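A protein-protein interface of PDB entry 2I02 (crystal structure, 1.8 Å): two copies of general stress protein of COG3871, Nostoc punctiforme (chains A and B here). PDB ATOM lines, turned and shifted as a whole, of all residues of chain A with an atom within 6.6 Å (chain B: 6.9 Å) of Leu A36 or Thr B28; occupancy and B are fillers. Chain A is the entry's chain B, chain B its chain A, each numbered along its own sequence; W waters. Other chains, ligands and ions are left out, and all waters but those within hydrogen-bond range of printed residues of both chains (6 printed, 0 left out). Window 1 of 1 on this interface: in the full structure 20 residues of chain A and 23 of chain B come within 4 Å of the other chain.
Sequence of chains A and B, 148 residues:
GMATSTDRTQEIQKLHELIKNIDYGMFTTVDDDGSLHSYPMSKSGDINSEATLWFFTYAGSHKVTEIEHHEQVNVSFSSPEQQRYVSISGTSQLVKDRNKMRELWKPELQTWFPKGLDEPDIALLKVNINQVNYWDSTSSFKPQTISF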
ATOM      1  N   THR A  28      30.807  -3.040  14.737  1.00  0.00           N
ATOM      2  CA  THR A  28      30.018  -4.013  13.981  1.00  0.00           C
ATOM      3  C   THR A  28      30.262  -5.447  14.422  1.00  0.00           C
ATOM      4  O   THR A  28      31.408  -5.868  14.549  1.00  0.00           O
ATOM      5  CB  THR A  28      30.256  -3.867  12.400  1.00  0.00           C
ATOM      6  OG1 THR A  28      30.084  -2.488  12.061  1.00  0.00           O
ATOM      7  CG2 THR A  28      29.262  -4.779  11.610  1.00  0.00           C
ATOM      8  N   THR A  29      29.158  -6.177  14.654  1.00  0.00           N
ATOM      9  CA  THR A  29      29.169  -7.563  15.048  1.00  0.00           C
ATOM     10  C   THR A  29      28.441  -8.424  14.010  1.00  0.00           C
ATOM     11  O   THR A  29      27.730  -7.892  13.145  1.00  0.00           O
ATOM     12  CB  THR A  29      28.391  -7.753  16.362  1.00  0.00           C
ATOM     13  OG1 THR A  29      27.009  -7.466  16.129  1.00  0.00           O
ATOM     14  CG2 THR A  29      28.886  -6.820  17.546  1.00  0.00           C
ATOM     15  N   VAL A  30      28.647  -9.729  14.122  1.00  0.00           N
ATOM     16  CA  VAL A  30      27.863 -10.701  13.345  1.00  0.00           C
ATOM     17  C   VAL A  30      27.165 -11.636  14.329  1.00  0.00           C
ATOM     18  O   VAL A  30      27.714 -12.024  15.351  1.00  0.00           O
ATOM     19  CB  VAL A  30      28.702 -11.446  12.272  1.00  0.00           C
ATOM     20  CG1 VAL A  30      29.795 -12.272  12.913  1.00  0.00           C
ATOM     21  CG2 VAL A  30      27.773 -12.291  11.293  1.00  0.00           C
ATOM     22  N   ASP A  31      25.901 -11.928  14.045  1.00  0.00           N
ATOM     23  CA  ASP A  31      25.072 -12.676  14.996  1.00  0.00           C
ATOM     24  C   ASP A  31      24.894 -14.129  14.535  1.00  0.00           C
ATOM     25  O   ASP A  31      25.425 -14.528  13.501  1.00  0.00           O
ATOM     26  CB  ASP A  31      23.742 -11.918  15.282  1.00  0.00           C
ATOM     27  CG  ASP A  31      22.746 -11.917  14.153  1.00  0.00           C
ATOM     28  OD1 ASP A  31      22.903 -12.645  13.161  1.00  0.00           O
ATOM     29  OD2 ASP A  31      21.753 -11.139  14.284  1.00  0.00           O
ATOM     30  N   GLY A  34      23.939 -14.779  11.094  1.00  0.00           N
ATOM     31  CA  GLY A  34      24.910 -14.205  10.142  1.00  0.00           C
ATOM     32  C   GLY A  34      24.682 -12.773   9.723  1.00  0.00           C
ATOM     33  O   GLY A  34      25.356 -12.278   8.837  1.00  0.00           O
ATOM     34  N   SER A  35      23.734 -12.098  10.360  1.00  0.00           N
ATOM     35  CA  SER A  35      23.466 -10.691  10.131  1.00  0.00           C
ATOM     36  C   SER A  35      24.501  -9.860  10.795  1.00  0.00           C
ATOM     37  O   SER A  35      24.994 -10.201  11.847  1.00  0.00           O
ATOM     38  CB  SER A  35      22.086 -10.314  10.624  1.00  0.00           C
ATOM     39  OG  SER A  35      21.117 -11.032   9.892  1.00  0.00           O
ATOM     40  N   LEU A  36      24.787  -8.709  10.182  1.00  0.00           N
ATOM     41  CA  LEU A  36      25.725  -7.761  10.759  1.00  0.00           C
ATOM     42  C   LEU A  36      25.011  -6.518  11.269  1.00  0.00           C
ATOM     43  O   LEU A  36      24.235  -5.867  10.525  1.00  0.00           O
ATOM     44  CB  LEU A  36      26.750  -7.361   9.692  1.00  0.00           C
ATOM     45  CG  LEU A  36      27.856  -8.359   9.386  1.00  0.00           C
ATOM     46  CD1 LEU A  36      27.366  -9.601   8.606  1.00  0.00           C
ATOM     47  CD2 LEU A  36      28.959  -7.606   8.597  1.00  0.00           C
ATOM     48  N   HIS A  37      25.255  -6.179  12.524  1.00  0.00           N
ATOM     49  CA  HIS A  37      24.648  -5.012  13.176  1.00  0.00           C
ATOM     50  C   HIS A  37      25.744  -4.081  13.596  1.00  0.00           C
ATOM     51  O   HIS A  37      26.746  -4.551  14.098  1.00  0.00           O
ATOM     52  CB  HIS A  37      23.876  -5.479  14.405  1.00  0.00           C
ATOM     53  CG  HIS A  37      22.677  -6.308  14.074  1.00  0.00           C
ATOM     54  ND1 HIS A  37      22.428  -7.526  14.679  1.00  0.00           N
ATOM     55  CD2 HIS A  37      21.664  -6.109  13.202  1.00  0.00           C
ATOM     56  CE1 HIS A  37      21.305  -8.033  14.198  1.00  0.00           C
ATOM     57  NE2 HIS A  37      20.823  -7.200  13.297  1.00  0.00           N
ATOM     58  N   SER A  38      25.552  -2.774  13.440  1.00  0.00           N
ATOM     59  CA  SER A  38      26.576  -1.806  13.902  1.00  0.00           C
ATOM     60  C   SER A  38      25.941  -0.837  14.899  1.00  0.00           C
ATOM     61  O   SER A  38      24.721  -0.575  14.905  1.00  0.00           O
ATOM     62  CB  SER A  38      27.137  -1.054  12.691  1.00  0.00           C
ATOM     63  OG  SER A  38      28.384  -0.469  12.945  1.00  0.00           O
ATOM     64  N   ASN A  74      34.416  -5.544  13.891  1.00  0.00           N
ATOM     65  CA  ASN A  74      35.049  -4.402  13.215  1.00  0.00           C
ATOM     66  C   ASN A  74      34.573  -3.125  13.870  1.00  0.00           C
ATOM     67  O   ASN A  74      33.410  -3.010  14.219  1.00  0.00           O
ATOM     68  CB  ASN A  74      34.719  -4.431  11.700  1.00  0.00           C
ATOM     69  CG  ASN A  74      35.373  -3.288  10.921  1.00  0.00           C
ATOM     70  OD1 ASN A  74      34.857  -2.171  10.906  1.00  0.00           O
ATOM     71  ND2 ASN A  74      36.490  -3.563  10.282  1.00  0.00           N
ATOM     72  N   SER A  76      34.637   0.905  12.813  1.00  0.00           N
ATOM     73  CA  SER A  76      35.034   1.889  11.819  1.00  0.00           C
ATOM     74  C   SER A  76      34.921   3.288  12.382  1.00  0.00           C
ATOM     75  O   SER A  76      34.073   3.567  13.254  1.00  0.00           O
ATOM     76  CB  SER A  76      34.190   1.786  10.566  1.00  0.00           C
ATOM     77  OG  SER A  76      32.850   2.137  10.849  1.00  0.00           O
ATOM     78  N   MET B  26      30.223   3.261   5.537  1.00  0.00           N
ATOM     79  CA  MET B  26      31.228   2.244   5.740  1.00  0.00           C
ATOM     80  C   MET B  26      30.529   0.903   5.532  1.00  0.00           C
ATOM     81  O   MET B  26      29.539   0.588   6.219  1.00  0.00           O
ATOM     82  CB  MET B  26      31.847   2.343   7.133  1.00  0.00           C
ATOM     83  CG  MET B  26      32.665   3.570   7.434  1.00  0.00           C
ATOM     84  SD  MET B  26      34.180   3.741   6.272  1.00  0.00           S
ATOM     85  CE  MET B  26      35.345   2.305   6.981  1.00  0.00           C
ATOM     86  N   PHE B  27      31.007   0.158   4.541  1.00  0.00           N
ATOM     87  CA  PHE B  27      30.436  -1.092   4.048  1.00  0.00           C
ATOM     88  C   PHE B  27      31.207  -2.236   4.636  1.00  0.00           C
ATOM     89  O   PHE B  27      32.419  -2.339   4.407  1.00  0.00           O
ATOM     90  CB  PHE B  27      30.550  -1.103   2.522  1.00  0.00           C
ATOM     91  CG  PHE B  27      29.758  -2.166   1.828  1.00  0.00           C
ATOM     92  CD1 PHE B  27      30.163  -3.479   1.866  1.00  0.00           C
ATOM     93  CD2 PHE B  27      28.628  -1.850   1.074  1.00  0.00           C
ATOM     94  CE1 PHE B  27      29.467  -4.456   1.210  1.00  0.00           C
ATOM     95  CE2 PHE B  27      27.919  -2.864   0.373  1.00  0.00           C
ATOM     96  CZ  PHE B  27      28.332  -4.160   0.463  1.00  0.00           C
ATOM     97  N   THR B  28      30.550  -3.050   5.477  1.00  0.00           N
ATOM     98  CA  THR B  28      31.224  -4.121   6.185  1.00  0.00           C
ATOM     99  C   THR B  28      30.800  -5.517   5.726  1.00  0.00           C
ATOM    100  O   THR B  28      29.601  -5.819   5.615  1.00  0.00           O
ATOM    101  CB  THR B  28      30.952  -4.035   7.713  1.00  0.00           C
ATOM    102  OG1 THR B  28      31.307  -2.723   8.184  1.00  0.00           O
ATOM    103  CG2 THR B  28      31.767  -5.075   8.485  1.00  0.00           C
ATOM    104  N   THR B  29      31.787  -6.382   5.555  1.00  0.00           N
ATOM    105  CA  THR B  29      31.606  -7.766   5.135  1.00  0.00           C
ATOM    106  C   THR B  29      32.323  -8.705   6.087  1.00  0.00           C
ATOM    107  O   THR B  29      33.131  -8.271   6.898  1.00  0.00           O
ATOM    108  CB  THR B  29      32.216  -8.012   3.711  1.00  0.00           C
ATOM    109  OG1 THR B  29      33.610  -7.679   3.743  1.00  0.00           O
ATOM    110  CG2 THR B  29      31.533  -7.221   2.618  1.00  0.00           C
ATOM    111  N   VAL B  30      32.042  -9.999   5.945  1.00  0.00           N
ATOM    112  CA  VAL B  30      32.691 -11.060   6.692  1.00  0.00           C
ATOM    113  C   VAL B  30      33.431 -11.921   5.717  1.00  0.00           C
ATOM    114  O   VAL B  30      32.895 -12.306   4.670  1.00  0.00           O
ATOM    115  CB  VAL B  30      31.700 -12.012   7.419  1.00  0.00           C
ATOM    116  CG1 VAL B  30      32.474 -12.917   8.401  1.00  0.00           C
ATOM    117  CG2 VAL B  30      30.622 -11.269   8.119  1.00  0.00           C
ATOM    118  N   LEU B  36      35.905  -9.406  10.038  1.00  0.00           N
ATOM    119  CA  LEU B  36      35.033  -8.398   9.460  1.00  0.00           C
ATOM    120  C   LEU B  36      35.897  -7.267   8.937  1.00  0.00           C
ATOM    121  O   LEU B  36      36.809  -6.839   9.629  1.00  0.00           O
ATOM    122  CB  LEU B  36      34.058  -7.830  10.457  1.00  0.00           C
ATOM    123  CG  LEU B  36      32.806  -8.620  10.758  1.00  0.00           C
ATOM    124  CD1 LEU B  36      33.191  -9.888  11.462  1.00  0.00           C
ATOM    125  CD2 LEU B  36      31.819  -7.777  11.583  1.00  0.00           C
ATOM    126  N   HIS B  37      35.608  -6.821   7.730  1.00  0.00           N
ATOM    127  CA  HIS B  37      36.362  -5.717   7.093  1.00  0.00           C
ATOM    128  C   HIS B  37      35.373  -4.681   6.609  1.00  0.00           C
ATOM    129  O   HIS B  37      34.299  -5.039   6.132  1.00  0.00           O
ATOM    130  CB  HIS B  37      37.175  -6.205   5.913  1.00  0.00           C
ATOM    131  CG  HIS B  37      38.165  -7.256   6.284  1.00  0.00           C
ATOM    132  ND1 HIS B  37      38.099  -8.540   5.801  1.00  0.00           N
ATOM    133  CD2 HIS B  37      39.232  -7.213   7.113  1.00  0.00           C
ATOM    134  CE1 HIS B  37      39.090  -9.249   6.316  1.00  0.00           C
ATOM    135  NE2 HIS B  37      39.785  -8.469   7.125  1.00  0.00           N
ATOM    136  N   SER B  38      35.734  -3.409   6.770  1.00  0.00           N
ATOM    137  CA  SER B  38      34.863  -2.310   6.318  1.00  0.00           C
ATOM    138  C   SER B  38      35.611  -1.419   5.341  1.00  0.00           C
ATOM    139  O   SER B  38      36.854  -1.300   5.380  1.00  0.00           O
ATOM    140  CB  SER B  38      34.251  -1.501   7.467  1.00  0.00           C
ATOM    141  OG  SER B  38      35.202  -0.798   8.237  1.00  0.00           O
ATOM    142  N   TYR B  39      34.832  -0.840   4.433  1.00  0.00           N
ATOM    143  CA  TYR B  39      35.313  -0.071   3.298  1.00  0.00           C
ATOM    144  C   TYR B  39      34.439   1.155   3.072  1.00  0.00           C
ATOM    145  O   TYR B  39      33.225   1.005   3.044  1.00  0.00           O
ATOM    146  CB  TYR B  39      35.170  -0.922   2.018  1.00  0.00           C
ATOM    147  CG  TYR B  39      35.678  -2.329   2.069  1.00  0.00           C
ATOM    148  CD1 TYR B  39      34.878  -3.380   2.501  1.00  0.00           C
ATOM    149  CD2 TYR B  39      36.946  -2.634   1.605  1.00  0.00           C
ATOM    150  CE1 TYR B  39      35.369  -4.683   2.547  1.00  0.00           C
ATOM    151  CE2 TYR B  39      37.437  -3.937   1.625  1.00  0.00           C
ATOM    152  CZ  TYR B  39      36.656  -4.961   2.093  1.00  0.00           C
ATOM    153  OH  TYR B  39      37.188  -6.252   2.089  1.00  0.00           O
ATOM    154  N   GLU B  66      34.012 -11.762  -0.908  1.00  0.00           N
ATOM    155  CA  GLU B  66      33.421 -11.953   0.417  1.00  0.00           C
ATOM    156  C   GLU B  66      31.917 -12.122   0.333  1.00  0.00           C
ATOM    157  O   GLU B  66      31.352 -13.067   0.919  1.00  0.00           O
ATOM    158  CB  GLU B  66      33.830 -10.804   1.369  1.00  0.00           C
ATOM    159  CG  GLU B  66      35.351 -10.760   1.553  1.00  0.00           C
ATOM    160  CD  GLU B  66      35.926  -9.507   2.213  1.00  0.00           C
ATOM    161  OE1 GLU B  66      35.395  -8.370   2.041  1.00  0.00           O
ATOM    162  OE2 GLU B  66      36.979  -9.671   2.884  1.00  0.00           O
ATOM    163  N   ILE B  67      31.253 -11.217  -0.376  1.00  0.00           N
ATOM    164  CA  ILE B  67      29.783 -11.243  -0.364  1.00  0.00           C
ATOM    165  C   ILE B  67      29.269 -12.468  -1.128  1.00  0.00           C
ATOM    166  O   ILE B  67      28.184 -12.978  -0.826  1.00  0.00           O
ATOM    167  CB  ILE B  67      29.116  -9.915  -0.813  1.00  0.00           C
ATOM    168  CG1 ILE B  67      29.433  -9.557  -2.272  1.00  0.00           C
ATOM    169  CG2 ILE B  67      29.487  -8.763   0.154  1.00  0.00           C
ATOM    170  CD1 ILE B  67      28.290  -9.842  -3.185  1.00  0.00           C
ATOM    171  N   HIS B  70      29.389 -14.870   1.804  1.00  0.00           N
ATOM    172  CA  HIS B  70      28.540 -14.440   2.917  1.00  0.00           C
ATOM    173  C   HIS B  70      27.814 -13.177   2.503  1.00  0.00           C
ATOM    174  O   HIS B  70      28.363 -12.096   2.591  1.00  0.00           O
ATOM    175  CB  HIS B  70      29.345 -14.206   4.194  1.00  0.00           C
ATOM    176  CG  HIS B  70      28.497 -14.101   5.423  1.00  0.00           C
ATOM    177  ND1 HIS B  70      28.023 -15.224   6.070  1.00  0.00           N
ATOM    178  CD2 HIS B  70      27.992 -13.039   6.093  1.00  0.00           C
ATOM    179  CE1 HIS B  70      27.280 -14.851   7.106  1.00  0.00           C
ATOM    180  NE2 HIS B  70      27.230 -13.532   7.136  1.00  0.00           N
ATOM    181  N   GLU B  71      26.576 -13.331   2.054  1.00  0.00           N
ATOM    182  CA  GLU B  71      25.833 -12.211   1.434  1.00  0.00           C
ATOM    183  C   GLU B  71      25.414 -11.126   2.404  1.00  0.00           C
ATOM    184  O   GLU B  71      25.182 -10.007   1.978  1.00  0.00           O
ATOM    185  CB  GLU B  71      24.613 -12.735   0.667  1.00  0.00           C
ATOM    186  CG  GLU B  71      23.535 -13.346   1.557  1.00  0.00           C
ATOM    187  CD  GLU B  71      22.213 -13.614   0.875  1.00  0.00           C
ATOM    188  OE1 GLU B  71      22.057 -13.315  -0.338  1.00  0.00           O
ATOM    189  OE2 GLU B  71      21.293 -14.101   1.589  1.00  0.00           O
ATOM    190  N   GLN B  72      25.266 -11.451   3.698  1.00  0.00           N
ATOM    191  CA  GLN B  72      24.890 -10.458   4.669  1.00  0.00           C
ATOM    192  C   GLN B  72      25.998  -9.426   4.841  1.00  0.00           C
ATOM    193  O   GLN B  72      27.177  -9.773   5.007  1.00  0.00           O
ATOM    194  CB  GLN B  72      24.578 -11.081   6.012  1.00  0.00           C
ATOM    195  CG  GLN B  72      23.467 -12.109   5.958  1.00  0.00           C
ATOM    196  CD  GLN B  72      24.006 -13.508   5.941  1.00  0.00           C
ATOM    197  OE1 GLN B  72      24.906 -13.851   5.163  1.00  0.00           O
ATOM    198  NE2 GLN B  72      23.461 -14.334   6.804  1.00  0.00           N
ATOM    199  N   VAL B  73      25.601  -8.166   4.864  1.00  0.00           N
ATOM    200  CA  VAL B  73      26.505  -7.040   5.047  1.00  0.00           C
ATOM    201  C   VAL B  73      25.899  -6.021   5.978  1.00  0.00           C
ATOM    202  O   VAL B  73      24.715  -6.090   6.304  1.00  0.00           O
ATOM    203  CB  VAL B  73      26.824  -6.353   3.680  1.00  0.00           C
ATOM    204  CG1 VAL B  73      27.520  -7.354   2.709  1.00  0.00           C
ATOM    205  CG2 VAL B  73      25.563  -5.662   3.039  1.00  0.00           C
ATOM    206  N   ASN B  74      26.700  -5.052   6.372  1.00  0.00           N
ATOM    207  CA  ASN B  74      26.178  -3.870   7.053  1.00  0.00           C
ATOM    208  C   ASN B  74      26.717  -2.660   6.367  1.00  0.00           C
ATOM    209  O   ASN B  74      27.864  -2.638   5.958  1.00  0.00           O
ATOM    210  CB  ASN B  74      26.640  -3.874   8.536  1.00  0.00           C
ATOM    211  CG  ASN B  74      26.087  -2.699   9.343  1.00  0.00           C
ATOM    212  OD1 ASN B  74      26.647  -1.593   9.331  1.00  0.00           O
ATOM    213  ND2 ASN B  74      24.958  -2.926   9.996  1.00  0.00           N
ATOM    214  N   VAL B  75      25.879  -1.639   6.251  1.00  0.00           N
ATOM    215  CA  VAL B  75      26.357  -0.334   5.828  1.00  0.00           C
ATOM    216  C   VAL B  75      26.006   0.652   6.907  1.00  0.00           C
ATOM    217  O   VAL B  75      24.838   0.742   7.298  1.00  0.00           O
ATOM    218  CB  VAL B  75      25.761   0.131   4.494  1.00  0.00           C
ATOM    219  CG1 VAL B  75      26.548   1.369   4.030  1.00  0.00           C
ATOM    220  CG2 VAL B  75      25.845  -0.978   3.446  1.00  0.00           C
ATOM    221  N   SER B  76      27.015   1.351   7.428  1.00  0.00           N
ATOM    222  CA  SER B  76      26.758   2.356   8.431  1.00  0.00           C
ATOM    223  C   SER B  76      26.949   3.763   7.858  1.00  0.00           C
ATOM    224  O   SER B  76      27.849   4.019   7.058  1.00  0.00           O
ATOM    225  CB  SER B  76      27.617   2.127   9.660  1.00  0.00           C
ATOM    226  OG  SER B  76      28.994   2.336   9.405  1.00  0.00           O
ATOM    227  N   SER B  87      22.665   2.291  11.180  1.00  0.00           N
ATOM    228  CA  SER B  87      23.174   0.961  10.839  1.00  0.00           C
ATOM    229  C   SER B  87      22.171   0.264   9.921  1.00  0.00           C
ATOM    230  O   SER B  87      21.023   0.055  10.318  1.00  0.00           O
ATOM    231  CB  SER B  87      23.319   0.155  12.089  1.00  0.00           C
ATOM    232  OG  SER B  87      23.588  -1.214  11.849  1.00  0.00           O
ATOM    233  N   ILE B  88      22.605  -0.127   8.738  1.00  0.00           N
ATOM    234  CA  ILE B  88      21.742  -0.803   7.782  1.00  0.00           C
ATOM    235  C   ILE B  88      22.200  -2.237   7.600  1.00  0.00           C
ATOM    236  O   ILE B  88      23.263  -2.474   7.056  1.00  0.00           O
ATOM    237  CB  ILE B  88      21.683  -0.067   6.430  1.00  0.00           C
ATOM    238  CG1 ILE B  88      21.155   1.359   6.659  1.00  0.00           C
ATOM    239  CG2 ILE B  88      20.818  -0.846   5.414  1.00  0.00           C
ATOM    240  CD1 ILE B  88      21.143   2.285   5.449  1.00  0.00           C
ATOM    241  N   SER B  89      21.384  -3.183   8.050  1.00  0.00           N
ATOM    242  CA  SER B  89      21.674  -4.613   7.839  1.00  0.00           C
ATOM    243  C   SER B  89      20.927  -5.047   6.619  1.00  0.00           C
ATOM    244  O   SER B  89      19.695  -4.850   6.530  1.00  0.00           O
ATOM    245  CB  SER B  89      21.211  -5.477   9.012  1.00  0.00           C
ATOM    246  OG  SER B  89      21.715  -4.979  10.250  1.00  0.00           O
ATOM    247  N   GLY B  90      21.638  -5.690   5.702  1.00  0.00           N
ATOM    248  CA  GLY B  90      21.045  -6.182   4.477  1.00  0.00           C
ATOM    249  C   GLY B  90      21.822  -7.327   3.863  1.00  0.00           C
ATOM    250  O   GLY B  90      22.823  -7.806   4.425  1.00  0.00           O
ATOM    251  N   GLN B 131      16.999  -4.548   7.914  1.00  0.00           N
ATOM    252  CA  GLN B 131      16.770  -3.812   9.160  1.00  0.00           C
ATOM    253  C   GLN B 131      17.597  -2.560   9.202  1.00  0.00           C
ATOM    254  O   GLN B 131      18.756  -2.526   8.735  1.00  0.00           O
ATOM    255  CB  GLN B 131      17.148  -4.711  10.341  1.00  0.00           C
ATOM    256  CG  GLN B 131      16.762  -4.196  11.707  1.00  0.00           C
ATOM    257  CD  GLN B 131      17.269  -5.103  12.834  1.00  0.00           C
ATOM    258  OE1 GLN B 131      18.071  -4.686  13.690  1.00  0.00           O
ATOM    259  NE2 GLN B 131      16.820  -6.337  12.825  1.00  0.00           N
ATOM    260  N   ASN B 133      18.742   0.273  12.087  1.00  0.00           N
ATOM    261  CA  ASN B 133      18.780   0.749  13.448  1.00  0.00           C
ATOM    262  C   ASN B 133      19.398   2.101  13.412  1.00  0.00           C
ATOM    263  O   ASN B 133      20.423   2.291  12.764  1.00  0.00           O
ATOM    264  CB  ASN B 133      19.585  -0.212  14.286  1.00  0.00           C
ATOM    265  CG  ASN B 133      18.933  -1.567  14.349  1.00  0.00           C
ATOM    266  OD1 ASN B 133      17.868  -1.709  14.928  1.00  0.00           O
ATOM    267  ND2 ASN B 133      19.538  -2.559  13.726  1.00  0.00           N
HETATM  268  O   HOH W   1      30.763   0.477  10.252  1.00  0.00           O
HETATM  269  O   HOH W   2      23.303  -8.223   7.737  1.00  0.00           O
HETATM  270  O   HOH W   3      22.561  -2.322  15.169  1.00  0.00           O
HETATM  271  O   HOH W   4      20.938 -13.112   8.167  1.00  0.00           O
HETATM  272  O   HOH W   5      19.042  -5.716  15.914  1.00  0.00           O
HETATM  273  O   HOH W   6      18.793  -7.453  11.641  1.00  0.00           O
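N of Thr B28 lies within hydrogen-bond range of O of Asn B74. OE1 of Gln B72 is in hydrogen-bond range of NE2 of His B70 (3.1 Å). The side-chain hydroxyl (OG) of Ser B87 lies within hydrogen-bond range of the side-chain amide nitrogen (ND2) of Asn B74, at 2.9 Å. The backbone NH of Ser B87 is in hydrogen-bond range of the backbone carbonyl oxygen of Asn B133 (2.7 Å). OG1 of Thr A28 is in hydrogen-bond range of OG of Ser A38, at 2.8 Å. The backbone NH of Thr A29 lies within hydrogen-bond range of the backbone carbonyl oxygen of His A37 (3.0 Å).
Thr A28 touches Leu B36. O of Thr B28 touches CD2 of Leu A36, 3.5 Å away. Leu A36 touches Val B30. Gln B72 touches Leu A36. His A37 touches Asn B74. C of His A37 touches OG of Ser B87, at 3.99 Å. CD2 of His A37 touches OG of Ser B89, 3.2 Å away. OE1 of Gln B131 touches NE2 of His A37, at 3.7 Å. His B37 touches Asn A74 (CA to ND2, 3.9 Å). Met B26 touches Ser A76.
Val A30 touches none of the printed residues of chain B. Of the printed residues of chain B, Leu A36 touches Thr B28 (3.5 Å), Val B30 (3.7 Å), Gln B72 (3.6 Å), Asn B74 (3.1 Å) and Ser B89 (2.7 Å). Printed residues of chain B within 4 Å of Ser A38: Asn B74 (3.4 Å) and Ser B87 (3.0 Å). Printed residues of chain A within 4 Å of Thr B28: Leu A36 (3.5 Å). Glu B71 touches none of the printed residues of chain A. Of the printed residues of chain A, Ser B89 touches Leu A36 (2.7 Å) and His A37 (3.2 Å). The nearest printed residue of chain B that does not touch Ser A38 is Ser B76 (4.3 Å).
Water W6 bridges NE2 of Gln B131 (2.6 Å) and NE2 of His A37 (2.6 Å). Water W5 lies within hydrogen-bond range of the side-chain amide oxygen (OE1) of Gln B131 and a ring nitrogen (NE2) of His A37. Water W1 lies within hydrogen-bond range of the side-chain hydroxyl (OG) of Ser B76 (2.7 Å) and the side-chain hydroxyl (OG) of Ser A76 (2.7 Å). Water W4 lies within hydrogen-bond range of OG of Ser A35 and NE2 of Gln B72. Water W3 lies within hydrogen-bond range of the backbone carbonyl oxygen of Ser A38 (2.8 Å) and the side-chain amide nitrogen of Asn B133 (3.4 Å). Water W2 lies within hydrogen-bond range of N of Leu A36, O of Val B73 and O of Gly B90.
Printed residues of chain B that touch a printed residue of chain A: Met B26, Thr B28, Val B30, Leu B36, His B37, Ser B38, His B70, Gln B72, Asn B74, Ser B87, Ser B89 and Gln B131. Among the printed residues, no Asp or Glu carboxylate lies within 4 Å of a Lys or Arg side-chain nitrogen of the other chain.
Leu A36 touches Val B30, but with the chains exchanged Val A30 does not touch Leu B36 (4.4 Å). Leu A36 touches Asn B74, and with the chains exchanged Asn A74 touches Leu B36. His A37 touches Asn B74, and with the chains exchanged Asn A74 touches His B37. Ser A76 touches Ser B38, but with the chains exchanged Ser A38 does not touch Ser B76 (4.3 Å). Positions printed for both chains: 28, 29, 30, 36, 37, 38, 74 and 76.
The backbone carbonyl oxygen (O) of Leu B36 is in hydrogen-bond range of the side-chain amide nitrogen (ND2) of Asn A74. The side-chain hydroxyl (OG) of Ser B38 lies within hydrogen-bond range of the side-chain amide oxygen (OD1) of Asn A74, 3.0 Å away. A ring nitrogen (NE2) of His B70 sits at hydrogen-bond distance from the backbone carbonyl oxygen (O) of Gly A34, 2.8 Å away. The side-chain amide nitrogen (NE2) of Gln B72 lies close to the backbone carbonyl oxygen (O) of Gly A34. The side-chain amide nitrogen (ND2) of Asn B74 sits at hydrogen-bond distance from the backbone carbonyl oxygen (O) of Leu A36. The side-chain amide nitrogen of Asn B74 sits close to the backbone NH of Ser A38 (3.5 Å). OG of Ser B87 lies within hydrogen-bond range of N of Ser A38 (3.0 Å). O of Leu A36 is in hydrogen-bond range of OG of Ser B89 (2.7 Å).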
